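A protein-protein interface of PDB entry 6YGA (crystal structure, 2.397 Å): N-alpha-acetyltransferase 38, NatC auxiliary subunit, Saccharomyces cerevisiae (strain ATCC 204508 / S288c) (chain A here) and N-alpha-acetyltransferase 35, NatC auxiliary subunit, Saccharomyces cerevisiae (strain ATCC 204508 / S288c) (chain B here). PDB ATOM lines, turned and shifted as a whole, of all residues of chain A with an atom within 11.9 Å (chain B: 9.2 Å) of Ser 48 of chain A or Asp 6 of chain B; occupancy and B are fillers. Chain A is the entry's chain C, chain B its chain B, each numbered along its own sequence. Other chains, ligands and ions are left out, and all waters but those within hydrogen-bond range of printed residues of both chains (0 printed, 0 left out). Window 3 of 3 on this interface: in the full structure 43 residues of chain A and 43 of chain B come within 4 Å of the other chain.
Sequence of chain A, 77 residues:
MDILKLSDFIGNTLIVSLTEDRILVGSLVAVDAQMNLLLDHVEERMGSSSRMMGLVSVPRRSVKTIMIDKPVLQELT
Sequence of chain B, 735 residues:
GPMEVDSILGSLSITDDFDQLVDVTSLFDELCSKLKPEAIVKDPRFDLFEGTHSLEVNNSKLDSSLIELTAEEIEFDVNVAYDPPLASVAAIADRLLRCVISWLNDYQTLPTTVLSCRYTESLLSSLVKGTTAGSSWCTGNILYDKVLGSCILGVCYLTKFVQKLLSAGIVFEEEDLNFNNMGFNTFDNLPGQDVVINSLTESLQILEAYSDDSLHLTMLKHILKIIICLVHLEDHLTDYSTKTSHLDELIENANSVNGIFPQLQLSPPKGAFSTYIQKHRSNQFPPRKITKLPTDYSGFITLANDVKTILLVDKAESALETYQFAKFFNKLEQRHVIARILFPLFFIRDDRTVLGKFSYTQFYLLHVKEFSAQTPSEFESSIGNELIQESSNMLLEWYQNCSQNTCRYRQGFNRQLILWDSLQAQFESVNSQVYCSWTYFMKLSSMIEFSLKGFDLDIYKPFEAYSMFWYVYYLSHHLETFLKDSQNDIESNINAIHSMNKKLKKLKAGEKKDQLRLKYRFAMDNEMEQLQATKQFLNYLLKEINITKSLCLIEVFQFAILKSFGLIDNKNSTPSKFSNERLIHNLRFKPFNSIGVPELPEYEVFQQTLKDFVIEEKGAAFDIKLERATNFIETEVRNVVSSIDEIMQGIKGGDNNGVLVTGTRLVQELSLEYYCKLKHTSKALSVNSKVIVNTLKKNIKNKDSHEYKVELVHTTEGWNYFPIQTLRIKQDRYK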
ATOM      1  N   ASP A  21       6.363  28.062   6.242  1.00  0.00           N
ATOM      2  CA  ASP A  21       5.980  27.574   7.562  1.00  0.00           C
ATOM      3  C   ASP A  21       6.948  28.020   8.649  1.00  0.00           C
ATOM      4  O   ASP A  21       6.626  27.904   9.835  1.00  0.00           O
ATOM      5  CB  ASP A  21       5.888  26.047   7.556  1.00  0.00           C
ATOM      6  CG  ASP A  21       4.885  25.530   6.551  1.00  0.00           C
ATOM      7  OD1 ASP A  21       4.315  26.353   5.804  1.00  0.00           O
ATOM      8  OD2 ASP A  21       4.664  24.300   6.508  1.00  0.00           O
ATOM      9  N   ARG A  22       8.119  28.526   8.273  1.00  0.00           N
ATOM     10  CA  ARG A  22       9.120  28.923   9.250  1.00  0.00           C
ATOM     11  C   ARG A  22       8.671  30.154  10.033  1.00  0.00           C
ATOM     12  O   ARG A  22       7.950  31.017   9.525  1.00  0.00           O
ATOM     13  CB  ARG A  22      10.456  29.196   8.557  1.00  0.00           C
ATOM     14  CG  ARG A  22      10.366  30.184   7.405  1.00  0.00           C
ATOM     15  CD  ARG A  22      11.623  30.180   6.538  1.00  0.00           C
ATOM     16  NE  ARG A  22      12.816  30.631   7.249  1.00  0.00           N
ATOM     17  CZ  ARG A  22      13.941  31.002   6.645  1.00  0.00           C
ATOM     18  NH1 ARG A  22      14.015  30.980   5.322  1.00  0.00           N
ATOM     19  NH2 ARG A  22      14.986  31.399   7.357  1.00  0.00           N
ATOM     20  N   ILE A  23       9.116  30.224  11.285  1.00  0.00           N
ATOM     21  CA  ILE A  23       8.833  31.337  12.184  1.00  0.00           C
ATOM     22  C   ILE A  23      10.133  31.756  12.857  1.00  0.00           C
ATOM     23  O   ILE A  23      10.956  30.905  13.219  1.00  0.00           O
ATOM     24  CB  ILE A  23       7.759  30.958  13.230  1.00  0.00           C
ATOM     25  CG1 ILE A  23       6.360  31.054  12.613  1.00  0.00           C
ATOM     26  CG2 ILE A  23       7.870  31.818  14.488  1.00  0.00           C
ATOM     27  CD1 ILE A  23       5.233  30.946  13.617  1.00  0.00           C
ATOM     28  N   GLU A  43      15.812  32.668  16.681  1.00  0.00           N
ATOM     29  CA  GLU A  43      15.524  31.240  16.679  1.00  0.00           C
ATOM     30  C   GLU A  43      14.559  30.946  15.540  1.00  0.00           C
ATOM     31  O   GLU A  43      13.471  31.531  15.480  1.00  0.00           O
ATOM     32  CB  GLU A  43      14.929  30.785  18.011  1.00  0.00           C
ATOM     33  CG  GLU A  43      14.562  29.310  18.039  1.00  0.00           C
ATOM     34  CD  GLU A  43      13.907  28.893  19.341  1.00  0.00           C
ATOM     35  OE1 GLU A  43      13.498  29.782  20.118  1.00  0.00           O
ATOM     36  OE2 GLU A  43      13.803  27.675  19.591  1.00  0.00           O
ATOM     37  N   GLU A  44      14.956  30.045  14.644  1.00  0.00           N
ATOM     38  CA  GLU A  44      14.134  29.641  13.510  1.00  0.00           C
ATOM     39  C   GLU A  44      13.389  28.360  13.866  1.00  0.00           C
ATOM     40  O   GLU A  44      14.010  27.314  14.079  1.00  0.00           O
ATOM     41  CB  GLU A  44      14.986  29.428  12.260  1.00  0.00           C
ATOM     42  CG  GLU A  44      14.168  29.260  10.984  1.00  0.00           C
ATOM     43  CD  GLU A  44      14.876  28.423   9.937  1.00  0.00           C
ATOM     44  OE1 GLU A  44      15.526  27.423  10.310  1.00  0.00           O
ATOM     45  OE2 GLU A  44      14.784  28.764   8.740  1.00  0.00           O
ATOM     46  N   ARG A  45      12.066  28.445  13.922  1.00  0.00           N
ATOM     47  CA  ARG A  45      11.209  27.314  14.254  1.00  0.00           C
ATOM     48  C   ARG A  45      10.474  26.855  13.000  1.00  0.00           C
ATOM     49  O   ARG A  45       9.757  27.643  12.375  1.00  0.00           O
ATOM     50  CB  ARG A  45      10.211  27.691  15.348  1.00  0.00           C
ATOM     51  CG  ARG A  45      10.839  27.990  16.701  1.00  0.00           C
ATOM     52  CD  ARG A  45       9.771  28.366  17.713  1.00  0.00           C
ATOM     53  NE  ARG A  45      10.336  28.780  18.993  1.00  0.00           N
ATOM     54  CZ  ARG A  45       9.628  29.325  19.977  1.00  0.00           C
ATOM     55  NH1 ARG A  45       8.325  29.523  19.823  1.00  0.00           N
ATOM     56  NH2 ARG A  45      10.218  29.676  21.111  1.00  0.00           N
ATOM     57  N   MET A  46      10.652  25.587  12.636  1.00  0.00           N
ATOM     58  CA  MET A  46       9.897  24.982  11.541  1.00  0.00           C
ATOM     59  C   MET A  46       9.302  23.651  11.980  1.00  0.00           C
ATOM     60  O   MET A  46      10.006  22.642  12.035  1.00  0.00           O
ATOM     61  CB  MET A  46      10.777  24.770  10.304  1.00  0.00           C
ATOM     62  CG  MET A  46      11.460  26.027   9.794  1.00  0.00           C
ATOM     63  SD  MET A  46      12.429  25.758   8.117  1.00  0.00           S
ATOM     64  CE  MET A  46      10.951  25.965   6.845  1.00  0.00           C
ATOM     65  N   GLY A  47       8.012  23.661  12.294  1.00  0.00           N
ATOM     66  CA  GLY A  47       7.339  22.441  12.708  1.00  0.00           C
ATOM     67  C   GLY A  47       7.954  21.910  13.986  1.00  0.00           C
ATOM     68  O   GLY A  47       7.876  22.537  15.048  1.00  0.00           O
ATOM     69  N   SER A  48       8.589  20.740  13.886  1.00  0.00           N
ATOM     70  CA  SER A  48       9.251  20.145  15.040  1.00  0.00           C
ATOM     71  C   SER A  48      10.622  20.755  15.297  1.00  0.00           C
ATOM     72  O   SER A  48      11.041  20.856  16.454  1.00  0.00           O
ATOM     73  CB  SER A  48       9.391  18.634  14.842  1.00  0.00           C
ATOM     74  OG  SER A  48      10.080  18.339  13.641  1.00  0.00           O
ATOM     75  N   SER A  49      11.324  21.180  14.251  1.00  0.00           N
ATOM     76  CA  SER A  49      12.726  21.545  14.383  1.00  0.00           C
ATOM     77  C   SER A  49      12.905  22.983  14.865  1.00  0.00           C
ATOM     78  O   SER A  49      12.061  23.858  14.640  1.00  0.00           O
ATOM     79  CB  SER A  49      13.457  21.347  13.053  1.00  0.00           C
ATOM     80  OG  SER A  49      13.693  19.969  12.802  1.00  0.00           O
ATOM     81  N   SER A  50      14.031  23.217  15.535  1.00  0.00           N
ATOM     82  CA  SER A  50      14.409  24.534  16.024  1.00  0.00           C
ATOM     83  C   SER A  50      15.916  24.691  15.894  1.00  0.00           C
ATOM     84  O   SER A  50      16.667  23.720  16.018  1.00  0.00           O
ATOM     85  CB  SER A  50      13.968  24.735  17.482  1.00  0.00           C
ATOM     86  OG  SER A  50      14.722  25.752  18.116  1.00  0.00           O
ATOM     87  N   ARG A  51      16.356  25.922  15.637  1.00  0.00           N
ATOM     88  CA  ARG A  51      17.780  26.189  15.484  1.00  0.00           C
ATOM     89  C   ARG A  51      18.035  27.681  15.631  1.00  0.00           C
ATOM     90  O   ARG A  51      17.149  28.510  15.406  1.00  0.00           O
ATOM     91  CB  ARG A  51      18.307  25.686  14.136  1.00  0.00           C
ATOM     92  CG  ARG A  51      17.775  26.437  12.925  1.00  0.00           C
ATOM     93  CD  ARG A  51      18.553  26.052  11.676  1.00  0.00           C
ATOM     94  NE  ARG A  51      18.279  26.937  10.547  1.00  0.00           N
ATOM     95  CZ  ARG A  51      19.119  27.128   9.532  1.00  0.00           C
ATOM     96  NH1 ARG A  51      20.288  26.500   9.511  1.00  0.00           N
ATOM     97  NH2 ARG A  51      18.795  27.947   8.541  1.00  0.00           N
ATOM     98  N   MET A  52      19.270  28.009  16.009  1.00  0.00           N
ATOM     99  CA  MET A  52      19.699  29.396  16.176  1.00  0.00           C
ATOM    100  C   MET A  52      20.363  29.915  14.904  1.00  0.00           C
ATOM    101  O   MET A  52      21.067  29.174  14.218  1.00  0.00           O
ATOM    102  CB  MET A  52      20.665  29.525  17.357  1.00  0.00           C
ATOM    103  CG  MET A  52      20.084  29.105  18.697  1.00  0.00           C
ATOM    104  SD  MET A  52      18.430  30.040  19.131  1.00  0.00           S
ATOM    105  CE  MET A  52      18.511  29.904  21.076  1.00  0.00           C
ATOM    106  N   PRO B   2       7.480  16.797   5.908  1.00  0.00           N
ATOM    107  CA  PRO B   2       6.079  17.211   5.768  1.00  0.00           C
ATOM    108  C   PRO B   2       5.118  16.145   6.274  1.00  0.00           C
ATOM    109  O   PRO B   2       4.399  16.381   7.244  1.00  0.00           O
ATOM    110  CB  PRO B   2       5.917  17.414   4.257  1.00  0.00           C
ATOM    111  CG  PRO B   2       7.307  17.616   3.742  1.00  0.00           C
ATOM    112  CD  PRO B   2       8.183  16.774   4.614  1.00  0.00           C
ATOM    113  N   MET B   3       5.117  14.985   5.624  1.00  0.00           N
ATOM    114  CA  MET B   3       4.206  13.899   5.978  1.00  0.00           C
ATOM    115  C   MET B   3       4.555  13.250   7.320  1.00  0.00           C
ATOM    116  O   MET B   3       3.737  12.521   7.889  1.00  0.00           O
ATOM    117  CB  MET B   3       4.187  12.826   4.872  1.00  0.00           C
ATOM    118  CG  MET B   3       3.310  13.171   3.664  1.00  0.00           C
ATOM    119  SD  MET B   3       2.934  11.679   2.431  1.00  0.00           S
ATOM    120  CE  MET B   3       2.419  10.303   3.711  1.00  0.00           C
ATOM    121  N   GLU B   4       5.760  13.515   7.824  1.00  0.00           N
ATOM    122  CA  GLU B   4       6.209  12.880   9.056  1.00  0.00           C
ATOM    123  C   GLU B   4       5.387  13.369  10.247  1.00  0.00           C
ATOM    124  O   GLU B   4       4.894  14.498  10.269  1.00  0.00           O
ATOM    125  CB  GLU B   4       7.695  13.147   9.299  1.00  0.00           C
ATOM    126  CG  GLU B   4       8.301  12.253  10.373  1.00  0.00           C
ATOM    127  CD  GLU B   4       9.580  12.806  10.961  1.00  0.00           C
ATOM    128  OE1 GLU B   4      10.337  13.473  10.226  1.00  0.00           O
ATOM    129  OE2 GLU B   4       9.825  12.571  12.164  1.00  0.00           O
ATOM    130  N   VAL B   5       5.252  12.499  11.248  1.00  0.00           N
ATOM    131  CA  VAL B   5       4.301  12.738  12.331  1.00  0.00           C
ATOM    132  C   VAL B   5       4.763  13.886  13.220  1.00  0.00           C
ATOM    133  O   VAL B   5       3.970  14.761  13.585  1.00  0.00           O
ATOM    134  CB  VAL B   5       4.093  11.454  13.151  1.00  0.00           C
ATOM    135  CG1 VAL B   5       2.874  11.598  14.052  1.00  0.00           C
ATOM    136  CG2 VAL B   5       3.950  10.249  12.232  1.00  0.00           C
ATOM    137  N   ASP B   6       6.050  13.900  13.580  1.00  0.00           N
ATOM    138  CA  ASP B   6       6.548  14.851  14.571  1.00  0.00           C
ATOM    139  C   ASP B   6       6.487  16.289  14.068  1.00  0.00           C
ATOM    140  O   ASP B   6       6.241  17.208  14.857  1.00  0.00           O
ATOM    141  CB  ASP B   6       7.978  14.481  14.976  1.00  0.00           C
ATOM    142  CG  ASP B   6       8.042  13.223  15.836  1.00  0.00           C
ATOM    143  OD1 ASP B   6       7.000  12.561  16.033  1.00  0.00           O
ATOM    144  OD2 ASP B   6       9.145  12.899  16.323  1.00  0.00           O
ATOM    145  N   SER B   7       6.701  16.504  12.768  1.00  0.00           N
ATOM    146  CA  SER B   7       6.570  17.847  12.212  1.00  0.00           C
ATOM    147  C   SER B   7       5.123  18.324  12.260  1.00  0.00           C
ATOM    148  O   SER B   7       4.863  19.513  12.478  1.00  0.00           O
ATOM    149  CB  SER B   7       7.105  17.875  10.781  1.00  0.00           C
ATOM    150  OG  SER B   7       6.554  16.827   9.998  1.00  0.00           O
ATOM    151  N   ILE B   8       4.171  17.408  12.065  1.00  0.00           N
ATOM    152  CA  ILE B   8       2.753  17.763  12.109  1.00  0.00           C
ATOM    153  C   ILE B   8       2.362  18.224  13.509  1.00  0.00           C
ATOM    154  O   ILE B   8       1.870  19.341  13.704  1.00  0.00           O
ATOM    155  CB  ILE B   8       1.888  16.575  11.651  1.00  0.00           C
ATOM    156  CG1 ILE B   8       2.154  16.239  10.180  1.00  0.00           C
ATOM    157  CG2 ILE B   8       0.414  16.871  11.862  1.00  0.00           C
ATOM    158  CD1 ILE B   8       1.627  14.878   9.760  1.00  0.00           C
ATOM    159  N   LEU B   9       2.576  17.362  14.507  1.00  0.00           N
ATOM    160  CA  LEU B   9       2.223  17.712  15.880  1.00  0.00           C
ATOM    161  C   LEU B   9       3.050  18.880  16.399  1.00  0.00           C
ATOM    162  O   LEU B   9       2.592  19.621  17.276  1.00  0.00           O
ATOM    163  CB  LEU B   9       2.396  16.501  16.797  1.00  0.00           C
ATOM    164  CG  LEU B   9       1.471  15.309  16.542  1.00  0.00           C
ATOM    165  CD1 LEU B   9       1.769  14.164  17.499  1.00  0.00           C
ATOM    166  CD2 LEU B   9       0.018  15.737  16.649  1.00  0.00           C
ATOM    167  N   GLY B  10       4.267  19.060  15.880  1.00  0.00           N
ATOM    168  CA  GLY B  10       5.131  20.124  16.359  1.00  0.00           C
ATOM    169  C   GLY B  10       4.624  21.517  16.053  1.00  0.00           C
ATOM    170  O   GLY B  10       5.041  22.477  16.711  1.00  0.00           O
ATOM    171  N   SER B  11       3.734  21.651  15.067  1.00  0.00           N
ATOM    172  CA  SER B  11       3.200  22.964  14.724  1.00  0.00           C
ATOM    173  C   SER B  11       2.390  23.550  15.874  1.00  0.00           C
ATOM    174  O   SER B  11       2.443  24.759  16.130  1.00  0.00           O
ATOM    175  CB  SER B  11       2.346  22.867  13.461  1.00  0.00           C
ATOM    176  OG  SER B  11       1.761  24.118  13.148  1.00  0.00           O
ATOM    177  N   LEU B  12       1.640  22.707  16.585  1.00  0.00           N
ATOM    178  CA  LEU B  12       0.848  23.192  17.710  1.00  0.00           C
ATOM    179  C   LEU B  12       1.730  23.628  18.875  1.00  0.00           C
ATOM    180  O   LEU B  12       1.339  24.510  19.647  1.00  0.00           O
ATOM    181  CB  LEU B  12      -0.129  22.109  18.162  1.00  0.00           C
ATOM    182  CG  LEU B  12      -0.933  21.430  17.051  1.00  0.00           C
ATOM    183  CD1 LEU B  12      -1.674  20.213  17.581  1.00  0.00           C
ATOM    184  CD2 LEU B  12      -1.902  22.410  16.404  1.00  0.00           C
ATOM    185  N   SER B  13       2.915  23.035  19.012  1.00  0.00           N
ATOM    186  CA  SER B  13       3.792  23.298  20.148  1.00  0.00           C
ATOM    187  C   SER B  13       4.653  24.540  19.970  1.00  0.00           C
ATOM    188  O   SER B  13       5.427  24.868  20.878  1.00  0.00           O
ATOM    189  CB  SER B  13       4.700  22.091  20.400  1.00  0.00           C
ATOM    190  OG  SER B  13       5.583  21.885  19.311  1.00  0.00           O
ATOM    191  N   ILE B  14       4.545  25.234  18.836  1.00  0.00           N
ATOM    192  CA  ILE B  14       5.431  26.363  18.568  1.00  0.00           C
ATOM    193  C   ILE B  14       5.118  27.528  19.498  1.00  0.00           C
ATOM    194  O   ILE B  14       6.025  28.173  20.037  1.00  0.00           O
ATOM    195  CB  ILE B  14       5.327  26.770  17.088  1.00  0.00           C
ATOM    196  CG1 ILE B  14       5.676  25.588  16.185  1.00  0.00           C
ATOM    197  CG2 ILE B  14       6.249  27.931  16.787  1.00  0.00           C
ATOM    198  CD1 ILE B  14       5.539  25.896  14.714  1.00  0.00           C
ATOM    199  N   HIS B 280      19.974  22.566   8.771  1.00  0.00           N
ATOM    200  CA  HIS B 280      19.168  22.175   9.920  1.00  0.00           C
ATOM    201  C   HIS B 280      19.842  22.419  11.262  1.00  0.00           C
ATOM    202  O   HIS B 280      19.162  22.772  12.230  1.00  0.00           O
ATOM    203  CB  HIS B 280      18.780  20.701   9.794  1.00  0.00           C
ATOM    204  CG  HIS B 280      17.824  20.428   8.674  1.00  0.00           C
ATOM    205  ND1 HIS B 280      18.235  20.051   7.413  1.00  0.00           N
ATOM    206  CD2 HIS B 280      16.473  20.490   8.626  1.00  0.00           C
ATOM    207  CE1 HIS B 280      17.177  19.885   6.640  1.00  0.00           C
ATOM    208  NE2 HIS B 280      16.096  20.145   7.352  1.00  0.00           N
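O of Glu 4 of chain B lies within hydrogen-bond range of OG of Ser 7 of chain B. The backbone carbonyl oxygen (O) of Gly 10 of chain B is in hydrogen-bond range of the side-chain hydroxyl (OG) of Ser 13 of chain B (2.7 Å). The backbone NH (N) of Arg 45 of chain A sits at hydrogen-bond distance from the backbone carbonyl oxygen (O) of Ile 23 of chain A, at 2.8 Å. OE1 of Glu 43 of chain A is in salt-bridge range of NH2 of Arg 45 of chain A, 3.4 Å away. The side-chain carboxylate of Glu 44 of chain A is in salt-bridge range of the guanidinium group of Arg 51 of chain A (2.8 Å).
The guanidinium group (NH1) of Arg 45 of chain A is in hydrogen-bond range of the backbone carbonyl oxygen (O) of Ile 14 of chain B (2.7 Å). The backbone carbonyl oxygen of Gly 47 of chain A sits close to the backbone carbonyl oxygen of Gly 10 of chain B.
Ser 48 of chain A touches just these residues of chain B: Asp 6 and Ser 7. Asp 6 of chain B touches one residue of chain A. Printed residues of chain B within 4 Å of Gly 47 of chain A: Ser 7, Gly 10 and Ile 14. Ser 49 of chain A touches none of the printed residues of chain B. No residue of chain A comes within 4 Å of Glu 4 of chain B. Ser 7 of chain B touches just these residues of chain A: Gly 47 (3.8 Å) and Ser 48 (3.8 Å). Gly 10 of chain B touches just one residue of chain A: Gly 47 (3.3 Å). No residue of chain A comes within 4 Å of Ser 11 of chain B. Of the printed residues of chain B, Arg 51 of chain A touches His 280 (3.4 Å). Of the printed residues of chain A, Ile 14 of chain B touches Arg 45 (2.7 Å) and Gly 47 (3.9 Å). Of the printed residues of chain A, His 280 of chain B touches Arg 51 (3.4 Å). Printed residues of chain B within 4 Å of Arg 45 of chain A: Ile 14.
Of the 13 printed residues of chain A, 4 touch a printed residue of chain B. Of the 14 printed residues of chain B, 5 touch a printed residue of chain A. Printed residues of chain B that touch a printed residue of chain A: Asp 6, Ser 7, Gly 10, Ile 14 and His 280. Along chain B the printed residues that touch a printed residue of chain A span positions 6 to 280. Among the printed residues, 7 pairs touch across the chains. Among the printed residues, no Asp or Glu carboxylate lies within 4 Å of a Lys or Arg side-chain nitrogen of the other chain.
CA of Gly 47 of chain A touches O of Ser 7 of chain B, 3.8 Å away. O of Gly 47 of chain A touches CG1 of Ile 14 of chain B, at 3.9 Å. Ser 48 of chain A touches Asp 6 of chain B. Ser 7 of chain B touches Ser 48 of chain A. Arg 51 of chain A touches His 280 of chain B (CD to O, 3.4 Å).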
